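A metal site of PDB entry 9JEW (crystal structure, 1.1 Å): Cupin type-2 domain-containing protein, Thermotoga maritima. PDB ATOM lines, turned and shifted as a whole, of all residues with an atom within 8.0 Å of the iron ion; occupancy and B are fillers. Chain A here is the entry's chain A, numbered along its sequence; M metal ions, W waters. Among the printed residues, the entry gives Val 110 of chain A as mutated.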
ATOM      1  N   LYS A  22      -8.580 -40.198 -22.231  1.00  0.00           N
ATOM      2  CA  LYS A  22      -9.514 -39.105 -22.316  1.00  0.00           C
ATOM      3  C   LYS A  22     -10.099 -38.920 -23.711  1.00  0.00           C
ATOM      4  O   LYS A  22     -10.804 -37.940 -23.926  1.00  0.00           O
ATOM      5  CB  LYS A  22      -8.925 -37.814 -21.739  1.00  0.00           C
ATOM      6  CG  LYS A  22      -7.625 -37.292 -22.309  1.00  0.00           C
ATOM      7  CD  LYS A  22      -7.175 -36.029 -21.571  1.00  0.00           C
ATOM      8  CE  LYS A  22      -5.906 -35.425 -22.114  1.00  0.00           C
ATOM      9  NZ  LYS A  22      -4.883 -36.426 -22.516  1.00  0.00           N
ATOM     10  N   ARG A  43      -3.478 -30.514 -38.143  1.00  0.00           N
ATOM     11  CA  ARG A  43      -4.027 -31.873 -38.147  1.00  0.00           C
ATOM     12  C   ARG A  43      -5.489 -31.827 -38.528  1.00  0.00           C
ATOM     13  O   ARG A  43      -6.178 -30.844 -38.257  1.00  0.00           O
ATOM     14  CB  ARG A  43      -3.840 -32.566 -36.813  1.00  0.00           C
ATOM     15  CG  ARG A  43      -2.395 -32.731 -36.410  1.00  0.00           C
ATOM     16  CD  ARG A  43      -1.669 -31.596 -35.812  1.00  0.00           C
ATOM     17  NE  ARG A  43      -2.492 -30.765 -35.007  1.00  0.00           N
ATOM     18  CZ  ARG A  43      -2.856 -31.089 -33.763  1.00  0.00           C
ATOM     19  NH1 ARG A  43      -2.509 -32.165 -33.151  1.00  0.00           N
ATOM     20  NH2 ARG A  43      -3.663 -30.220 -33.228  1.00  0.00           N
ATOM     21  N   PHE A  45      -8.831 -33.905 -37.669  1.00  0.00           N
ATOM     22  CA  PHE A  45      -9.420 -34.865 -36.745  1.00  0.00           C
ATOM     23  C   PHE A  45     -10.759 -35.334 -37.318  1.00  0.00           C
ATOM     24  O   PHE A  45     -11.534 -34.551 -37.841  1.00  0.00           O
ATOM     25  CB  PHE A  45      -9.656 -34.267 -35.380  1.00  0.00           C
ATOM     26  CG  PHE A  45      -8.503 -34.161 -34.460  1.00  0.00           C
ATOM     27  CD1 PHE A  45      -8.687 -34.555 -33.144  1.00  0.00           C
ATOM     28  CD2 PHE A  45      -7.269 -33.669 -34.800  1.00  0.00           C
ATOM     29  CE1 PHE A  45      -7.664 -34.480 -32.244  1.00  0.00           C
ATOM     30  CE2 PHE A  45      -6.233 -33.623 -33.912  1.00  0.00           C
ATOM     31  CZ  PHE A  45      -6.384 -34.095 -32.636  1.00  0.00           C
ATOM     32  N   ILE A  53     -13.981 -36.531 -26.970  1.00  0.00           N
ATOM     33  CA  ILE A  53     -12.768 -35.942 -26.417  1.00  0.00           C
ATOM     34  C   ILE A  53     -13.187 -35.287 -25.129  1.00  0.00           C
ATOM     35  O   ILE A  53     -13.867 -34.254 -25.100  1.00  0.00           O
ATOM     36  CB  ILE A  53     -12.161 -34.949 -27.418  1.00  0.00           C
ATOM     37  CG1 ILE A  53     -11.729 -35.634 -28.717  1.00  0.00           C
ATOM     38  CG2 ILE A  53     -11.010 -34.193 -26.779  1.00  0.00           C
ATOM     39  CD1 ILE A  53     -11.407 -34.708 -29.871  1.00  0.00           C
ATOM     40  N   ASP A  54     -12.855 -35.922 -23.989  1.00  0.00           N
ATOM     41  CA  ASP A  54     -13.313 -35.433 -22.704  1.00  0.00           C
ATOM     42  C   ASP A  54     -12.802 -34.026 -22.448  1.00  0.00           C
ATOM     43  O   ASP A  54     -11.736 -33.629 -22.941  1.00  0.00           O
ATOM     44  CB  ASP A  54     -12.733 -36.280 -21.566  1.00  0.00           C
ATOM     45  CG  ASP A  54     -13.172 -37.702 -21.493  1.00  0.00           C
ATOM     46  OD1 ASP A  54     -14.205 -38.050 -22.105  1.00  0.00           O
ATOM     47  OD2 ASP A  54     -12.534 -38.426 -20.691  1.00  0.00           O
ATOM     48  N   ARG A  55     -13.495 -33.295 -21.598  1.00  0.00           N
ATOM     49  CA  ARG A  55     -13.029 -31.995 -21.130  1.00  0.00           C
ATOM     50  C   ARG A  55     -11.598 -32.094 -20.589  1.00  0.00           C
ATOM     51  O   ARG A  55     -11.293 -33.006 -19.796  1.00  0.00           O
ATOM     52  CB  ARG A  55     -13.948 -31.448 -20.035  1.00  0.00           C
ATOM     53  CG  ARG A  55     -15.281 -30.938 -20.528  1.00  0.00           C
ATOM     54  CD  ARG A  55     -16.119 -30.399 -19.374  1.00  0.00           C
ATOM     55  NE  ARG A  55     -17.357 -29.839 -19.850  1.00  0.00           N
ATOM     56  CZ  ARG A  55     -18.473 -30.458 -20.157  1.00  0.00           C
ATOM     57  NH1 ARG A  55     -18.546 -31.770 -20.030  1.00  0.00           N
ATOM     58  NH2 ARG A  55     -19.507 -29.772 -20.633  1.00  0.00           N
ATOM     59  N   HIS A  56     -10.769 -31.181 -21.019  1.00  0.00           N
ATOM     60  CA  HIS A  56      -9.377 -31.132 -20.632  1.00  0.00           C
ATOM     61  C   HIS A  56      -8.880 -29.720 -20.899  1.00  0.00           C
ATOM     62  O   HIS A  56      -9.575 -28.859 -21.457  1.00  0.00           O
ATOM     63  CB  HIS A  56      -8.535 -32.144 -21.440  1.00  0.00           C
ATOM     64  CG  HIS A  56      -8.491 -31.775 -22.882  1.00  0.00           C
ATOM     65  ND1 HIS A  56      -9.531 -31.967 -23.783  1.00  0.00           N
ATOM     66  CD2 HIS A  56      -7.533 -31.177 -23.607  1.00  0.00           C
ATOM     67  CE1 HIS A  56      -9.127 -31.520 -24.967  1.00  0.00           C
ATOM     68  NE2 HIS A  56      -7.906 -31.007 -24.909  1.00  0.00           N
ATOM     69  N   SER A  57      -7.637 -29.476 -20.493  1.00  0.00           N
ATOM     70  CA  SER A  57      -6.992 -28.217 -20.814  1.00  0.00           C
ATOM     71  C   SER A  57      -5.481 -28.469 -20.982  1.00  0.00           C
ATOM     72  O   SER A  57      -4.970 -29.497 -20.519  1.00  0.00           O
ATOM     73  CB  SER A  57      -7.255 -27.156 -19.748  1.00  0.00           C
ATOM     74  OG  SER A  57      -6.707 -27.535 -18.516  1.00  0.00           O
ATOM     75  N   HIS A  58      -4.803 -27.538 -21.606  1.00  0.00           N
ATOM     76  CA  HIS A  58      -3.370 -27.640 -21.830  1.00  0.00           C
ATOM     77  C   HIS A  58      -2.799 -26.224 -21.955  1.00  0.00           C
ATOM     78  O   HIS A  58      -3.541 -25.307 -22.274  1.00  0.00           O
ATOM     79  CB  HIS A  58      -2.973 -28.520 -23.004  1.00  0.00           C
ATOM     80  CG  HIS A  58      -3.979 -28.432 -24.071  1.00  0.00           C
ATOM     81  ND1 HIS A  58      -4.300 -27.290 -24.783  1.00  0.00           N
ATOM     82  CD2 HIS A  58      -4.858 -29.391 -24.525  1.00  0.00           C
ATOM     83  CE1 HIS A  58      -5.286 -27.560 -25.597  1.00  0.00           C
ATOM     84  NE2 HIS A  58      -5.669 -28.832 -25.498  1.00  0.00           N
ATOM     85  N   TRP A  60      -1.374 -24.463 -24.132  1.00  0.00           N
ATOM     86  CA  TRP A  60      -1.320 -23.925 -25.465  1.00  0.00           C
ATOM     87  C   TRP A  60      -2.768 -23.771 -25.960  1.00  0.00           C
ATOM     88  O   TRP A  60      -3.679 -24.466 -25.493  1.00  0.00           O
ATOM     89  CB  TRP A  60      -0.521 -24.766 -26.456  1.00  0.00           C
ATOM     90  CG  TRP A  60      -0.959 -26.177 -26.590  1.00  0.00           C
ATOM     91  CD1 TRP A  60      -1.966 -26.711 -27.362  1.00  0.00           C
ATOM     92  CD2 TRP A  60      -0.405 -27.293 -25.865  1.00  0.00           C
ATOM     93  NE1 TRP A  60      -2.039 -28.067 -27.177  1.00  0.00           N
ATOM     94  CE2 TRP A  60      -1.104 -28.449 -26.267  1.00  0.00           C
ATOM     95  CE3 TRP A  60       0.628 -27.434 -24.953  1.00  0.00           C
ATOM     96  CZ2 TRP A  60      -0.795 -29.720 -25.763  1.00  0.00           C
ATOM     97  CZ3 TRP A  60       0.931 -28.691 -24.443  1.00  0.00           C
ATOM     98  CH2 TRP A  60       0.219 -29.815 -24.855  1.00  0.00           C
ATOM     99  N   GLU A  61      -2.930 -22.856 -26.917  1.00  0.00           N
ATOM    100  CA  GLU A  61      -4.188 -22.587 -27.597  1.00  0.00           C
ATOM    101  C   GLU A  61      -4.518 -23.637 -28.655  1.00  0.00           C
ATOM    102  O   GLU A  61      -3.655 -24.361 -29.119  1.00  0.00           O
ATOM    103  CB  GLU A  61      -4.115 -21.214 -28.236  1.00  0.00           C
ATOM    104  CG  GLU A  61      -3.183 -21.055 -29.421  1.00  0.00           C
ATOM    105  CD  GLU A  61      -1.722 -20.838 -29.185  1.00  0.00           C
ATOM    106  OE1 GLU A  61      -1.242 -21.069 -28.041  1.00  0.00           O
ATOM    107  OE2 GLU A  61      -1.027 -20.428 -30.138  1.00  0.00           O
ATOM    108  N   HIS A  62      -5.781 -23.616 -29.067  1.00  0.00           N
ATOM    109  CA  HIS A  62      -6.239 -24.288 -30.278  1.00  0.00           C
ATOM    110  C   HIS A  62      -6.872 -23.281 -31.223  1.00  0.00           C
ATOM    111  O   HIS A  62      -7.640 -22.421 -30.806  1.00  0.00           O
ATOM    112  CB  HIS A  62      -7.294 -25.366 -30.078  1.00  0.00           C
ATOM    113  CG  HIS A  62      -6.978 -26.575 -29.342  1.00  0.00           C
ATOM    114  ND1 HIS A  62      -6.068 -27.491 -29.763  1.00  0.00           N
ATOM    115  CD2 HIS A  62      -7.585 -27.225 -28.333  1.00  0.00           C
ATOM    116  CE1 HIS A  62      -6.029 -28.528 -28.976  1.00  0.00           C
ATOM    117  NE2 HIS A  62      -6.947 -28.402 -28.042  1.00  0.00           N
ATOM    118  N   ILE A  64      -9.328 -23.893 -34.548  1.00  0.00           N
ATOM    119  CA  ILE A  64     -10.096 -24.986 -35.146  1.00  0.00           C
ATOM    120  C   ILE A  64     -10.998 -24.456 -36.250  1.00  0.00           C
ATOM    121  O   ILE A  64     -11.554 -23.381 -36.119  1.00  0.00           O
ATOM    122  CB  ILE A  64     -10.936 -25.667 -34.041  1.00  0.00           C
ATOM    123  CG1 ILE A  64     -10.004 -26.410 -33.079  1.00  0.00           C
ATOM    124  CG2 ILE A  64     -11.983 -26.595 -34.576  1.00  0.00           C
ATOM    125  CD1 ILE A  64     -10.671 -26.887 -31.817  1.00  0.00           C
ATOM    126  N   VAL A  90      -9.696 -21.584 -28.857  1.00  0.00           N
ATOM    127  CA  VAL A  90      -9.601 -22.017 -27.468  1.00  0.00           C
ATOM    128  C   VAL A  90      -8.338 -21.395 -26.856  1.00  0.00           C
ATOM    129  O   VAL A  90      -7.256 -21.667 -27.318  1.00  0.00           O
ATOM    130  CB  VAL A  90      -9.569 -23.535 -27.331  1.00  0.00           C
ATOM    131  CG1 VAL A  90      -9.674 -23.905 -25.840  1.00  0.00           C
ATOM    132  CG2 VAL A  90     -10.623 -24.222 -28.162  1.00  0.00           C
ATOM    133  N   GLU A  94      -7.885 -23.080 -21.251  1.00  0.00           N
ATOM    134  CA  GLU A  94      -9.343 -23.071 -21.205  1.00  0.00           C
ATOM    135  C   GLU A  94      -9.846 -24.499 -21.305  1.00  0.00           C
ATOM    136  O   GLU A  94      -9.361 -25.284 -22.138  1.00  0.00           O
ATOM    137  CB  GLU A  94      -9.876 -22.240 -22.384  1.00  0.00           C
ATOM    138  CG  GLU A  94     -11.380 -22.124 -22.488  1.00  0.00           C
ATOM    139  CD  GLU A  94     -11.807 -20.985 -23.392  1.00  0.00           C
ATOM    140  OE1 GLU A  94     -11.192 -20.607 -24.423  1.00  0.00           O
ATOM    141  OE2 GLU A  94     -12.913 -20.458 -23.082  1.00  0.00           O
ATOM    142  N   ILE A  95     -10.790 -24.870 -20.460  1.00  0.00           N
ATOM    143  CA  ILE A  95     -11.382 -26.197 -20.492  1.00  0.00           C
ATOM    144  C   ILE A  95     -12.215 -26.367 -21.760  1.00  0.00           C
ATOM    145  O   ILE A  95     -13.020 -25.500 -22.139  1.00  0.00           O
ATOM    146  CB  ILE A  95     -12.220 -26.442 -19.243  1.00  0.00           C
ATOM    147  CG1 ILE A  95     -11.308 -26.454 -18.003  1.00  0.00           C
ATOM    148  CG2 ILE A  95     -13.026 -27.716 -19.326  1.00  0.00           C
ATOM    149  CD1 ILE A  95     -12.086 -26.189 -16.726  1.00  0.00           C
ATOM    150  N   HIS A  96     -12.028 -27.506 -22.440  1.00  0.00           N
ATOM    151  CA  HIS A  96     -12.742 -27.781 -23.682  1.00  0.00           C
ATOM    152  C   HIS A  96     -12.779 -29.274 -23.930  1.00  0.00           C
ATOM    153  O   HIS A  96     -11.889 -30.002 -23.480  1.00  0.00           O
ATOM    154  CB  HIS A  96     -12.068 -27.060 -24.871  1.00  0.00           C
ATOM    155  CG  HIS A  96     -10.661 -27.490 -25.115  1.00  0.00           C
ATOM    156  ND1 HIS A  96      -9.651 -27.120 -24.253  1.00  0.00           N
ATOM    157  CD2 HIS A  96     -10.043 -28.271 -26.057  1.00  0.00           C
ATOM    158  CE1 HIS A  96      -8.507 -27.656 -24.649  1.00  0.00           C
ATOM    159  NE2 HIS A  96      -8.714 -28.401 -25.719  1.00  0.00           N
ATOM    160  N   GLY A  97     -13.743 -29.711 -24.709  1.00  0.00           N
ATOM    161  CA  GLY A  97     -13.803 -31.075 -25.181  1.00  0.00           C
ATOM    162  C   GLY A  97     -14.770 -31.123 -26.352  1.00  0.00           C
ATOM    163  O   GLY A  97     -15.306 -30.074 -26.746  1.00  0.00           O
ATOM    164  N   PHE A  98     -15.008 -32.320 -26.898  1.00  0.00           N
ATOM    165  CA  PHE A  98     -15.817 -32.438 -28.102  1.00  0.00           C
ATOM    166  C   PHE A  98     -16.572 -33.761 -28.077  1.00  0.00           C
ATOM    167  O   PHE A  98     -16.074 -34.755 -27.561  1.00  0.00           O
ATOM    168  CB  PHE A  98     -14.961 -32.377 -29.362  1.00  0.00           C
ATOM    169  CG  PHE A  98     -14.133 -31.135 -29.439  1.00  0.00           C
ATOM    170  CD1 PHE A  98     -14.675 -29.939 -29.853  1.00  0.00           C
ATOM    171  CD2 PHE A  98     -12.806 -31.145 -29.016  1.00  0.00           C
ATOM    172  CE1 PHE A  98     -13.921 -28.752 -29.861  1.00  0.00           C
ATOM    173  CE2 PHE A  98     -12.050 -29.994 -29.033  1.00  0.00           C
ATOM    174  CZ  PHE A  98     -12.619 -28.781 -29.417  1.00  0.00           C
ATOM    175  N   VAL A 110      -7.453 -28.826 -36.636  1.00  0.00           N
ATOM    176  CA  VAL A 110      -7.002 -28.360 -35.341  1.00  0.00           C
ATOM    177  C   VAL A 110      -5.530 -27.995 -35.488  1.00  0.00           C
ATOM    178  O   VAL A 110      -4.714 -28.832 -35.875  1.00  0.00           O
ATOM    179  CB  VAL A 110      -7.092 -29.390 -34.204  1.00  0.00           C
ATOM    180  CG1 VAL A 110      -6.665 -28.723 -32.882  1.00  0.00           C
ATOM    181  CG2 VAL A 110      -8.478 -29.995 -34.087  1.00  0.00           C
ATOM    182  N   ILE A 112      -2.187 -26.107 -33.492  1.00  0.00           N
ATOM    183  CA  ILE A 112      -1.590 -25.764 -32.200  1.00  0.00           C
ATOM    184  C   ILE A 112      -0.168 -25.302 -32.472  1.00  0.00           C
ATOM    185  O   ILE A 112       0.464 -25.720 -33.458  1.00  0.00           O
ATOM    186  CB  ILE A 112      -1.585 -26.951 -31.219  1.00  0.00           C
ATOM    187  CG1 ILE A 112      -0.778 -28.166 -31.717  1.00  0.00           C
ATOM    188  CG2 ILE A 112      -3.017 -27.324 -30.891  1.00  0.00           C
ATOM    189  CD1 ILE A 112      -0.660 -29.267 -30.670  1.00  0.00           C
HETATM  190 FE    FE M   1      -7.282 -29.703 -26.468  1.00  0.00          FE
HETATM  191  O   HOH W   1      -8.684 -30.668 -27.766  1.00  0.00           O
HETATM  192  O   HOH W   2      -5.964 -31.140 -27.180  1.00  0.00           O
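The backbone carbonyl oxygen (O) of His 62 is in hydrogen-bond range of the backbone NH (N) of Val 90, at 3.0 Å. ND1 of His 58 is in hydrogen-bond range of O of Trp 60 (3.0 Å). ND1 of His 96 is in hydrogen-bond range of O of Glu 94. The backbone carbonyl oxygen (O) of Asp 54 is in hydrogen-bond range of a ring nitrogen (ND1) of His 56 (2.9 Å).
The iron ion is bound by NE2 of His 62 (2.1 Å), NE2 of His 58 (2.1 Å), NE2 of His 96 (2.1 Å), water W2 (2.1 Å), NE2 of His 56 (2.1 Å) and water W1 (2.1 Å).
Within 4 Å of the iron ion: His 56, His 58, His 62 and His 96.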
